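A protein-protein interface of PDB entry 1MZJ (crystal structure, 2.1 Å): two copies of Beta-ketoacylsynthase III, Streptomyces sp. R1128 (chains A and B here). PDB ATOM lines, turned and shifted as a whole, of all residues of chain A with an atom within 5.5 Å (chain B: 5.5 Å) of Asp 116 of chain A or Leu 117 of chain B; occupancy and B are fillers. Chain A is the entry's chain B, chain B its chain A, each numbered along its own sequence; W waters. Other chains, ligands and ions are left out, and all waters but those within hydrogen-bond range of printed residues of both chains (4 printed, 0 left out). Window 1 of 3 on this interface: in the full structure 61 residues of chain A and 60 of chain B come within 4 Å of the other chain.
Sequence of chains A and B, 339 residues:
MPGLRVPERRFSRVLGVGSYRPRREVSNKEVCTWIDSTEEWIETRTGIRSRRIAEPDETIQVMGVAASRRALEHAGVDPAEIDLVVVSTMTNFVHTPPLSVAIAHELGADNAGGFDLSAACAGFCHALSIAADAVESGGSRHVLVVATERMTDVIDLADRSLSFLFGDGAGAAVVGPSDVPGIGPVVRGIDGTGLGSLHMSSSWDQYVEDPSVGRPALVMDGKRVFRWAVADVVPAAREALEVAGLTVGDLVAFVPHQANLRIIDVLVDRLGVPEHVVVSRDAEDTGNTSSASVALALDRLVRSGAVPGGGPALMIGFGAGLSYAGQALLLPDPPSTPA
The backbone NH (N) of Asp 116 of chain B sits at hydrogen-bond distance from the backbone carbonyl oxygen (O) of Ser 118 of chain A (2.7 Å).
The backbone carbonyl oxygen (O) of Asp 116 of chain A sits at hydrogen-bond distance from the backbone NH (N) of Ser 118 of chain B (3.0 Å).
N of Leu 117 of chain B sits at hydrogen-bond distance from O of Val 87 of chain B.
N of Thr 89 of chain B sits at hydrogen-bond distance from O of Leu 117 of chain B (3.0 Å).
O of Phe 115 of chain A is in hydrogen-bond range of N of Val 87 of chain A, at 3.3 Å.
The backbone carbonyl oxygen (O) of Val 87 of chain A is in hydrogen-bond range of the backbone NH (N) of Leu 117 of chain A (2.6 Å).
The backbone NH (N) of Leu 99 of chain A lies within hydrogen-bond range of the side-chain carboxylate (OD2) of Asp 116 of chain A, at 2.6 Å.
OG of Ser 100 of chain A sits close to N of Phe 115 of chain A (3.5 Å).
CB of Pro 98 of chain A touches O of Ser 118 of chain B, at 3.7 Å.
Pro 98 of chain A touches Ala 119 of chain B (CG to CA, 3.5 Å).
His 126 of chain B touches Gly 114 of chain A.
Ser 118 of chain B touches Phe 115 of chain A (O to CA, 3.9 Å).
CB of Ala 119 of chain B touches CB of Phe 115 of chain A, 3.7 Å away.
His 126 of chain B touches Phe 115 of chain A (CG to CD1, 3.7 Å).
Phe 115 of chain A touches Ile 130 of chain B (CZ to CD1, 3.7 Å).
Leu 117 of chain B touches Asp 116 of chain A (CA to O, 3.7 Å).
Phe 115 of chain B touches Leu 117 of chain A (CD2 to CD1, 3.5 Å).
Leu 117 of chain A touches Asp 116 of chain B.
Printed residues of chain B within 4 Å of Asp 116 of chain A: Leu 117 (3.7 Å) and Ser 118 (3.0 Å).
Of chain A, only Phe 115 (3.7 Å) and Asp 116 (3.7 Å) come within 4 Å of Leu 117 of chain B.
Printed residues of chain A within 4 Å of Ile 130 of chain B: Phe 115.
Of the printed residues of chain B, Pro 98 of chain A touches Ser 118 (3.7 Å) and Ala 119 (3.5 Å).
Of the printed residues of chain B, Leu 117 of chain A touches Phe 115 and Asp 116.
Printed residues of chain A within 4 Å of Ser 118 of chain B: Pro 98, Phe 115 and Asp 116.
Printed residues of chain A within 4 Å of His 126 of chain B: Gly 114 (3.95 Å) and Phe 115 (3.7 Å).
Asn 92 of chain A touches none of the printed residues of chain B.
The nearest residue of chain B that does not touch Asp 116 of chain A is Asp 116 of chain B (4.1 Å).
The nearest printed residue of chain A that does not touch Ser 118 of chain B is Leu 117 of chain A (4.9 Å).
Of the 15 printed residues of chain A, 6 touch a printed residue of chain B.
Printed residues of chain A that touch a printed residue of chain B: Pro 98, Gly 114, Phe 115, Asp 116, Leu 117 and Ser 118.
Printed residues of chain B that touch a printed residue of chain A: Phe 115, Asp 116, Leu 117, Ser 118, Ala 119, His 126 and Ile 130.
Among the printed residues, 14 pairs touch across the chains.
Among the printed residues, no Asp or Glu carboxylate lies within 4 Å of a Lys or Arg side-chain nitrogen of the other chain.
Phe 115 of chain A touches Leu 117 of chain B, and with the chains exchanged Leu 117 of chain A touches Phe 115 of chain B.
Phe 115 of chain A touches Ser 118 of chain B, and with the chains exchanged Ser 118 of chain A touches Phe 115 of chain B.
Asp 116 of chain A touches Leu 117 of chain B, and with the chains exchanged Leu 117 of chain A touches Asp 116 of chain B.
Asp 116 of chain A touches Ser 118 of chain B, and with the chains exchanged Ser 118 of chain A touches Asp 116 of chain B.
Positions printed for both chains: 86, 87, 88, 89, 115, 116, 117 and 118.
Of the 14 pairs that touch across the chains among the printed residues, 8 have their exchanged pair printed and touching as well.
Water W1 lies within hydrogen-bond range of OG of Ser 118 of chain A (2.8 Å) and OD2 of Asp 116 of chain B (3.3 Å).
Water W4 lies within hydrogen-bond range of the side-chain hydroxyl (OG) of Ser 118 of chain B (2.8 Å) and the side-chain carboxylate (OD2) of Asp 116 of chain A (3.1 Å).
Water W3 lies within hydrogen-bond range of NE2 of His 126 of chain B and O of Gly 114 of chain A.
Water W2 lies within hydrogen-bond range of the backbone NH (N) of Gly 114 of chain A (3.1 Å) and a ring nitrogen (NE2) of His 126 of chain B (3.3 Å).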
ATOM      1  N   VAL A  86     -20.521  -7.961 -23.359  1.00  0.00           N
ATOM      2  CA  VAL A  86     -20.660  -6.596 -23.874  1.00  0.00           C
ATOM      3  C   VAL A  86     -20.420  -6.667 -25.384  1.00  0.00           C
ATOM      4  O   VAL A  86     -19.367  -7.096 -25.831  1.00  0.00           O
ATOM      5  CB  VAL A  86     -19.643  -5.597 -23.278  1.00  0.00           C
ATOM      6  CG1 VAL A  86     -19.846  -4.175 -23.902  1.00  0.00           C
ATOM      7  CG2 VAL A  86     -19.794  -5.536 -21.731  1.00  0.00           C
ATOM      8  N   VAL A  87     -21.427  -6.293 -26.157  1.00  0.00           N
ATOM      9  CA  VAL A  87     -21.307  -6.294 -27.597  1.00  0.00           C
ATOM     10  C   VAL A  87     -21.325  -4.847 -28.104  1.00  0.00           C
ATOM     11  O   VAL A  87     -22.216  -4.048 -27.796  1.00  0.00           O
ATOM     12  CB  VAL A  87     -22.481  -7.072 -28.258  1.00  0.00           C
ATOM     13  CG1 VAL A  87     -22.371  -6.993 -29.776  1.00  0.00           C
ATOM     14  CG2 VAL A  87     -22.483  -8.549 -27.801  1.00  0.00           C
ATOM     15  N   SER A  88     -20.312  -4.531 -28.893  1.00  0.00           N
ATOM     16  CA  SER A  88     -20.136  -3.250 -29.496  1.00  0.00           C
ATOM     17  C   SER A  88     -20.510  -3.370 -30.962  1.00  0.00           C
ATOM     18  O   SER A  88     -19.987  -4.237 -31.697  1.00  0.00           O
ATOM     19  CB  SER A  88     -18.678  -2.862 -29.386  1.00  0.00           C
ATOM     20  OG  SER A  88     -18.465  -1.675 -30.081  1.00  0.00           O
ATOM     21  N   THR A  89     -21.427  -2.526 -31.399  1.00  0.00           N
ATOM     22  CA  THR A  89     -21.820  -2.543 -32.791  1.00  0.00           C
ATOM     23  C   THR A  89     -22.553  -1.270 -33.126  1.00  0.00           C
ATOM     24  O   THR A  89     -23.091  -0.617 -32.225  1.00  0.00           O
ATOM     25  CB  THR A  89     -22.787  -3.719 -33.111  1.00  0.00           C
ATOM     26  OG1 THR A  89     -23.111  -3.720 -34.526  1.00  0.00           O
ATOM     27  CG2 THR A  89     -24.068  -3.600 -32.256  1.00  0.00           C
ATOM     28  N   ASN A  92     -26.734  -2.569 -36.105  1.00  0.00           N
ATOM     29  CA  ASN A  92     -27.784  -3.476 -35.681  1.00  0.00           C
ATOM     30  C   ASN A  92     -29.095  -2.806 -35.985  1.00  0.00           C
ATOM     31  O   ASN A  92     -29.310  -1.707 -35.539  1.00  0.00           O
ATOM     32  CB  ASN A  92     -27.652  -3.689 -34.176  1.00  0.00           C
ATOM     33  CG  ASN A  92     -28.569  -4.776 -33.623  1.00  0.00           C
ATOM     34  OD1 ASN A  92     -28.471  -5.079 -32.434  1.00  0.00           O
ATOM     35  ND2 ASN A  92     -29.453  -5.357 -34.443  1.00  0.00           N
ATOM     36  N   PRO A  97     -34.573  -7.354 -28.356  1.00  0.00           N
ATOM     37  CA  PRO A  97     -33.728  -7.209 -27.161  1.00  0.00           C
ATOM     38  C   PRO A  97     -32.288  -7.054 -27.598  1.00  0.00           C
ATOM     39  O   PRO A  97     -32.002  -7.225 -28.783  1.00  0.00           O
ATOM     40  CB  PRO A  97     -33.967  -8.513 -26.398  1.00  0.00           C
ATOM     41  CG  PRO A  97     -34.343  -9.527 -27.514  1.00  0.00           C
ATOM     42  CD  PRO A  97     -35.157  -8.710 -28.493  1.00  0.00           C
ATOM     43  N   PRO A  98     -31.345  -6.775 -26.641  1.00  0.00           N
ATOM     44  CA  PRO A  98     -29.916  -6.601 -26.928  1.00  0.00           C
ATOM     45  C   PRO A  98     -29.271  -7.818 -27.602  1.00  0.00           C
ATOM     46  O   PRO A  98     -29.546  -9.000 -27.223  1.00  0.00           O
ATOM     47  CB  PRO A  98     -29.272  -6.354 -25.548  1.00  0.00           C
ATOM     48  CG  PRO A  98     -30.423  -5.944 -24.658  1.00  0.00           C
ATOM     49  CD  PRO A  98     -31.595  -6.739 -25.183  1.00  0.00           C
ATOM     50  N   LEU A  99     -28.415  -7.516 -28.593  1.00  0.00           N
ATOM     51  CA  LEU A  99     -27.671  -8.542 -29.311  1.00  0.00           C
ATOM     52  C   LEU A  99     -26.838  -9.326 -28.288  1.00  0.00           C
ATOM     53  O   LEU A  99     -26.770 -10.575 -28.351  1.00  0.00           O
ATOM     54  CB  LEU A  99     -26.688  -7.912 -30.317  1.00  0.00           C
ATOM     55  CG  LEU A  99     -26.435  -8.660 -31.624  1.00  0.00           C
ATOM     56  CD1 LEU A  99     -25.144  -8.084 -32.197  1.00  0.00           C
ATOM     57  CD2 LEU A  99     -26.374 -10.140 -31.435  1.00  0.00           C
ATOM     58  N   SER A 100     -26.182  -8.602 -27.379  1.00  0.00           N
ATOM     59  CA  SER A 100     -25.358  -9.245 -26.360  1.00  0.00           C
ATOM     60  C   SER A 100     -26.094 -10.393 -25.605  1.00  0.00           C
ATOM     61  O   SER A 100     -25.463 -11.383 -25.261  1.00  0.00           O
ATOM     62  CB  SER A 100     -24.893  -8.212 -25.342  1.00  0.00           C
ATOM     63  OG  SER A 100     -26.060  -7.635 -24.782  1.00  0.00           O
ATOM     64  N   VAL A 101     -27.418 -10.277 -25.402  1.00  0.00           N
ATOM     65  CA  VAL A 101     -28.199 -11.298 -24.667  1.00  0.00           C
ATOM     66  C   VAL A 101     -28.426 -12.554 -25.545  1.00  0.00           C
ATOM     67  O   VAL A 101     -28.408 -13.685 -25.067  1.00  0.00           O
ATOM     68  CB  VAL A 101     -29.585 -10.703 -24.174  1.00  0.00           C
ATOM     69  CG1 VAL A 101     -30.389 -11.715 -23.385  1.00  0.00           C
ATOM     70  CG2 VAL A 101     -29.337  -9.538 -23.307  1.00  0.00           C
ATOM     71  N   GLY A 114     -25.856  -8.698 -20.020  1.00  0.00           N
ATOM     72  CA  GLY A 114     -25.357  -8.136 -21.229  1.00  0.00           C
ATOM     73  C   GLY A 114     -26.082  -6.871 -21.632  1.00  0.00           C
ATOM     74  O   GLY A 114     -27.299  -6.813 -21.679  1.00  0.00           O
ATOM     75  N   PHE A 115     -25.275  -5.835 -21.918  1.00  0.00           N
ATOM     76  CA  PHE A 115     -25.737  -4.779 -22.779  1.00  0.00           C
ATOM     77  C   PHE A 115     -25.000  -4.817 -24.118  1.00  0.00           C
ATOM     78  O   PHE A 115     -23.804  -4.998 -24.199  1.00  0.00           O
ATOM     79  CB  PHE A 115     -25.615  -3.417 -22.054  1.00  0.00           C
ATOM     80  CG  PHE A 115     -24.249  -3.231 -21.451  1.00  0.00           C
ATOM     81  CD1 PHE A 115     -23.975  -3.671 -20.150  1.00  0.00           C
ATOM     82  CD2 PHE A 115     -23.266  -2.632 -22.206  1.00  0.00           C
ATOM     83  CE1 PHE A 115     -22.692  -3.502 -19.626  1.00  0.00           C
ATOM     84  CE2 PHE A 115     -21.979  -2.487 -21.676  1.00  0.00           C
ATOM     85  CZ  PHE A 115     -21.709  -2.896 -20.389  1.00  0.00           C
ATOM     86  N   ASP A 116     -25.581  -4.036 -25.023  1.00  0.00           N
ATOM     87  CA  ASP A 116     -24.875  -3.654 -26.266  1.00  0.00           C
ATOM     88  C   ASP A 116     -24.362  -2.253 -26.044  1.00  0.00           C
ATOM     89  O   ASP A 116     -24.877  -1.494 -25.225  1.00  0.00           O
ATOM     90  CB  ASP A 116     -25.793  -3.657 -27.512  1.00  0.00           C
ATOM     91  CG  ASP A 116     -26.485  -5.002 -27.737  1.00  0.00           C
ATOM     92  OD1 ASP A 116     -25.997  -5.974 -27.160  1.00  0.00           O
ATOM     93  OD2 ASP A 116     -27.515  -5.106 -28.479  1.00  0.00           O
ATOM     94  N   LEU A 117     -23.379  -1.892 -26.823  1.00  0.00           N
ATOM     95  CA  LEU A 117     -22.743  -0.615 -26.666  1.00  0.00           C
ATOM     96  C   LEU A 117     -22.629  -0.031 -28.071  1.00  0.00           C
ATOM     97  O   LEU A 117     -22.421  -0.755 -29.047  1.00  0.00           O
ATOM     98  CB  LEU A 117     -21.385  -0.883 -26.004  1.00  0.00           C
ATOM     99  CG  LEU A 117     -20.569   0.325 -25.659  1.00  0.00           C
ATOM    100  CD1 LEU A 117     -19.895   0.031 -24.320  1.00  0.00           C
ATOM    101  CD2 LEU A 117     -19.539   0.656 -26.786  1.00  0.00           C
ATOM    102  N   SER A 118     -22.818   1.267 -28.175  1.00  0.00           N
ATOM    103  CA  SER A 118     -22.737   1.912 -29.469  1.00  0.00           C
ATOM    104  C   SER A 118     -21.890   3.166 -29.312  1.00  0.00           C
ATOM    105  O   SER A 118     -22.313   4.080 -28.616  1.00  0.00           O
ATOM    106  CB  SER A 118     -24.138   2.284 -29.946  1.00  0.00           C
ATOM    107  OG  SER A 118     -24.058   2.816 -31.257  1.00  0.00           O
ATOM    108  N   VAL B  86     -22.727   8.398 -20.382  1.00  0.00           N
ATOM    109  CA  VAL B  86     -23.238   7.107 -20.823  1.00  0.00           C
ATOM    110  C   VAL B  86     -24.735   7.330 -21.086  1.00  0.00           C
ATOM    111  O   VAL B  86     -25.488   7.784 -20.223  1.00  0.00           O
ATOM    112  CB  VAL B  86     -23.122   6.002 -19.752  1.00  0.00           C
ATOM    113  CG1 VAL B  86     -23.614   4.692 -20.340  1.00  0.00           C
ATOM    114  CG2 VAL B  86     -21.684   5.873 -19.222  1.00  0.00           C
ATOM    115  N   VAL B  87     -25.165   7.045 -22.291  1.00  0.00           N
ATOM    116  CA  VAL B  87     -26.582   7.243 -22.563  1.00  0.00           C
ATOM    117  C   VAL B  87     -27.295   5.916 -22.828  1.00  0.00           C
ATOM    118  O   VAL B  87     -26.919   5.130 -23.687  1.00  0.00           O
ATOM    119  CB  VAL B  87     -26.709   8.150 -23.787  1.00  0.00           C
ATOM    120  CG1 VAL B  87     -28.096   7.993 -24.409  1.00  0.00           C
ATOM    121  CG2 VAL B  87     -26.503   9.598 -23.386  1.00  0.00           C
ATOM    122  N   SER B  88     -28.338   5.660 -22.016  1.00  0.00           N
ATOM    123  CA  SER B  88     -29.105   4.433 -22.198  1.00  0.00           C
ATOM    124  C   SER B  88     -30.415   4.700 -22.940  1.00  0.00           C
ATOM    125  O   SER B  88     -31.211   5.558 -22.576  1.00  0.00           O
ATOM    126  CB  SER B  88     -29.398   3.845 -20.816  1.00  0.00           C
ATOM    127  OG  SER B  88     -30.357   2.795 -20.945  1.00  0.00           O
ATOM    128  N   THR B  89     -30.610   3.953 -24.042  1.00  0.00           N
ATOM    129  CA  THR B  89     -31.814   4.154 -24.838  1.00  0.00           C
ATOM    130  C   THR B  89     -31.982   3.060 -25.893  1.00  0.00           C
ATOM    131  O   THR B  89     -31.027   2.527 -26.442  1.00  0.00           O
ATOM    132  CB  THR B  89     -31.704   5.516 -25.525  1.00  0.00           C
ATOM    133  OG1 THR B  89     -32.922   5.784 -26.222  1.00  0.00           O
ATOM    134  CG2 THR B  89     -30.551   5.501 -26.533  1.00  0.00           C
ATOM    135  N   MET B  90     -33.255   2.700 -26.138  1.00  0.00           N
ATOM    136  CA  MET B  90     -33.536   1.701 -27.160  1.00  0.00           C
ATOM    137  C   MET B  90     -34.460   2.256 -28.247  1.00  0.00           C
ATOM    138  O   MET B  90     -34.978   1.540 -29.094  1.00  0.00           O
ATOM    139  CB  MET B  90     -34.185   0.493 -26.486  1.00  0.00           C
ATOM    140  CG  MET B  90     -35.589   0.798 -25.960  1.00  0.00           C
ATOM    141  SD  MET B  90     -36.410  -0.667 -25.320  1.00  0.00           S
ATOM    142  CE  MET B  90     -37.233  -1.173 -26.838  1.00  0.00           C
ATOM    143  N   PHE B 115     -20.357   6.805 -24.599  1.00  0.00           N
ATOM    144  CA  PHE B 115     -20.931   5.882 -25.570  1.00  0.00           C
ATOM    145  C   PHE B 115     -22.381   5.533 -25.225  1.00  0.00           C
ATOM    146  O   PHE B 115     -22.833   5.657 -24.093  1.00  0.00           O
ATOM    147  CB  PHE B 115     -20.079   4.612 -25.582  1.00  0.00           C
ATOM    148  CG  PHE B 115     -19.864   4.134 -24.176  1.00  0.00           C
ATOM    149  CD1 PHE B 115     -18.712   4.505 -23.493  1.00  0.00           C
ATOM    150  CD2 PHE B 115     -20.816   3.336 -23.563  1.00  0.00           C
ATOM    151  CE1 PHE B 115     -18.517   4.076 -22.188  1.00  0.00           C
ATOM    152  CE2 PHE B 115     -20.613   2.910 -22.253  1.00  0.00           C
ATOM    153  CZ  PHE B 115     -19.465   3.277 -21.562  1.00  0.00           C
ATOM    154  N   ASP B 116     -23.130   5.120 -26.263  1.00  0.00           N
ATOM    155  CA  ASP B 116     -24.531   4.784 -26.046  1.00  0.00           C
ATOM    156  C   ASP B 116     -24.693   3.352 -25.529  1.00  0.00           C
ATOM    157  O   ASP B 116     -23.982   2.433 -25.914  1.00  0.00           O
ATOM    158  CB  ASP B 116     -25.271   4.944 -27.375  1.00  0.00           C
ATOM    159  CG  ASP B 116     -25.362   6.423 -27.725  1.00  0.00           C
ATOM    160  OD1 ASP B 116     -24.895   7.231 -26.923  1.00  0.00           O
ATOM    161  OD2 ASP B 116     -25.899   6.748 -28.781  1.00  0.00           O
ATOM    162  N   LEU B 117     -25.644   3.190 -24.591  1.00  0.00           N
ATOM    163  CA  LEU B 117     -25.900   1.861 -24.050  1.00  0.00           C
ATOM    164  C   LEU B 117     -27.311   1.379 -24.393  1.00  0.00           C
ATOM    165  O   LEU B 117     -28.281   2.125 -24.371  1.00  0.00           O
ATOM    166  CB  LEU B 117     -25.724   1.923 -22.531  1.00  0.00           C
ATOM    167  CG  LEU B 117     -25.584   0.535 -21.902  1.00  0.00           C
ATOM    168  CD1 LEU B 117     -24.647   0.535 -20.694  1.00  0.00           C
ATOM    169  CD2 LEU B 117     -26.917  -0.031 -21.411  1.00  0.00           C
ATOM    170  N   SER B 118     -27.397   0.087 -24.760  1.00  0.00           N
ATOM    171  CA  SER B 118     -28.697  -0.448 -25.146  1.00  0.00           C
ATOM    172  C   SER B 118     -28.962  -1.808 -24.496  1.00  0.00           C
ATOM    173  O   SER B 118     -28.404  -2.832 -24.868  1.00  0.00           O
ATOM    174  CB  SER B 118     -28.723  -0.585 -26.669  1.00  0.00           C
ATOM    175  OG  SER B 118     -30.028  -0.990 -27.084  1.00  0.00           O
ATOM    176  N   ALA B 119     -29.820  -1.786 -23.459  1.00  0.00           N
ATOM    177  CA  ALA B 119     -30.141  -3.026 -22.763  1.00  0.00           C
ATOM    178  C   ALA B 119     -31.604  -3.056 -22.314  1.00  0.00           C
ATOM    179  O   ALA B 119     -31.936  -3.413 -21.191  1.00  0.00           O
ATOM    180  CB  ALA B 119     -29.221  -3.142 -21.548  1.00  0.00           C
ATOM    181  N   GLY B 123     -31.262  -0.958 -18.905  1.00  0.00           N
ATOM    182  CA  GLY B 123     -30.225   0.011 -19.285  1.00  0.00           C
ATOM    183  C   GLY B 123     -29.699   0.933 -18.214  1.00  0.00           C
ATOM    184  O   GLY B 123     -28.474   1.058 -18.069  1.00  0.00           O
ATOM    185  N   HIS B 126     -27.493  -0.928 -15.699  1.00  0.00           N
ATOM    186  CA  HIS B 126     -26.157  -1.297 -16.230  1.00  0.00           C
ATOM    187  C   HIS B 126     -25.310  -0.004 -16.290  1.00  0.00           C
ATOM    188  O   HIS B 126     -24.115  -0.030 -15.914  1.00  0.00           O
ATOM    189  CB  HIS B 126     -26.168  -1.887 -17.663  1.00  0.00           C
ATOM    190  CG  HIS B 126     -26.722  -3.276 -17.776  1.00  0.00           C
ATOM    191  ND1 HIS B 126     -26.091  -4.377 -17.224  1.00  0.00           N
ATOM    192  CD2 HIS B 126     -27.860  -3.740 -18.371  1.00  0.00           C
ATOM    193  CE1 HIS B 126     -26.820  -5.459 -17.469  1.00  0.00           C
ATOM    194  NE2 HIS B 126     -27.894  -5.104 -18.163  1.00  0.00           N
ATOM    195  N   ALA B 127     -25.906   1.116 -16.736  1.00  0.00           N
ATOM    196  CA  ALA B 127     -25.088   2.358 -16.882  1.00  0.00           C
ATOM    197  C   ALA B 127     -24.538   2.840 -15.570  1.00  0.00           C
ATOM    198  O   ALA B 127     -23.381   3.238 -15.470  1.00  0.00           O
ATOM    199  CB  ALA B 127     -25.860   3.467 -17.563  1.00  0.00           C
ATOM    200  N   ILE B 130     -21.545   0.881 -14.587  1.00  0.00           N
ATOM    201  CA  ILE B 130     -20.362   1.336 -15.404  1.00  0.00           C
ATOM    202  C   ILE B 130     -19.767   2.634 -14.806  1.00  0.00           C
ATOM    203  O   ILE B 130     -18.559   2.787 -14.654  1.00  0.00           O
ATOM    204  CB  ILE B 130     -20.789   1.614 -16.814  1.00  0.00           C
ATOM    205  CG1 ILE B 130     -21.104   0.285 -17.483  1.00  0.00           C
ATOM    206  CG2 ILE B 130     -19.698   2.365 -17.586  1.00  0.00           C
ATOM    207  CD1 ILE B 130     -21.938   0.447 -18.711  1.00  0.00           C
HETATM  208  O   HOH W   1     -24.883   5.422 -31.637  1.00  0.00           O
HETATM  209  O   HOH W   2     -28.064  -8.418 -17.915  1.00  0.00           O
HETATM  210  O   HOH W   3     -29.594  -6.406 -20.020  1.00  0.00           O
HETATM  211  O   HOH W   4     -30.236  -3.646 -27.865  1.00  0.00           O
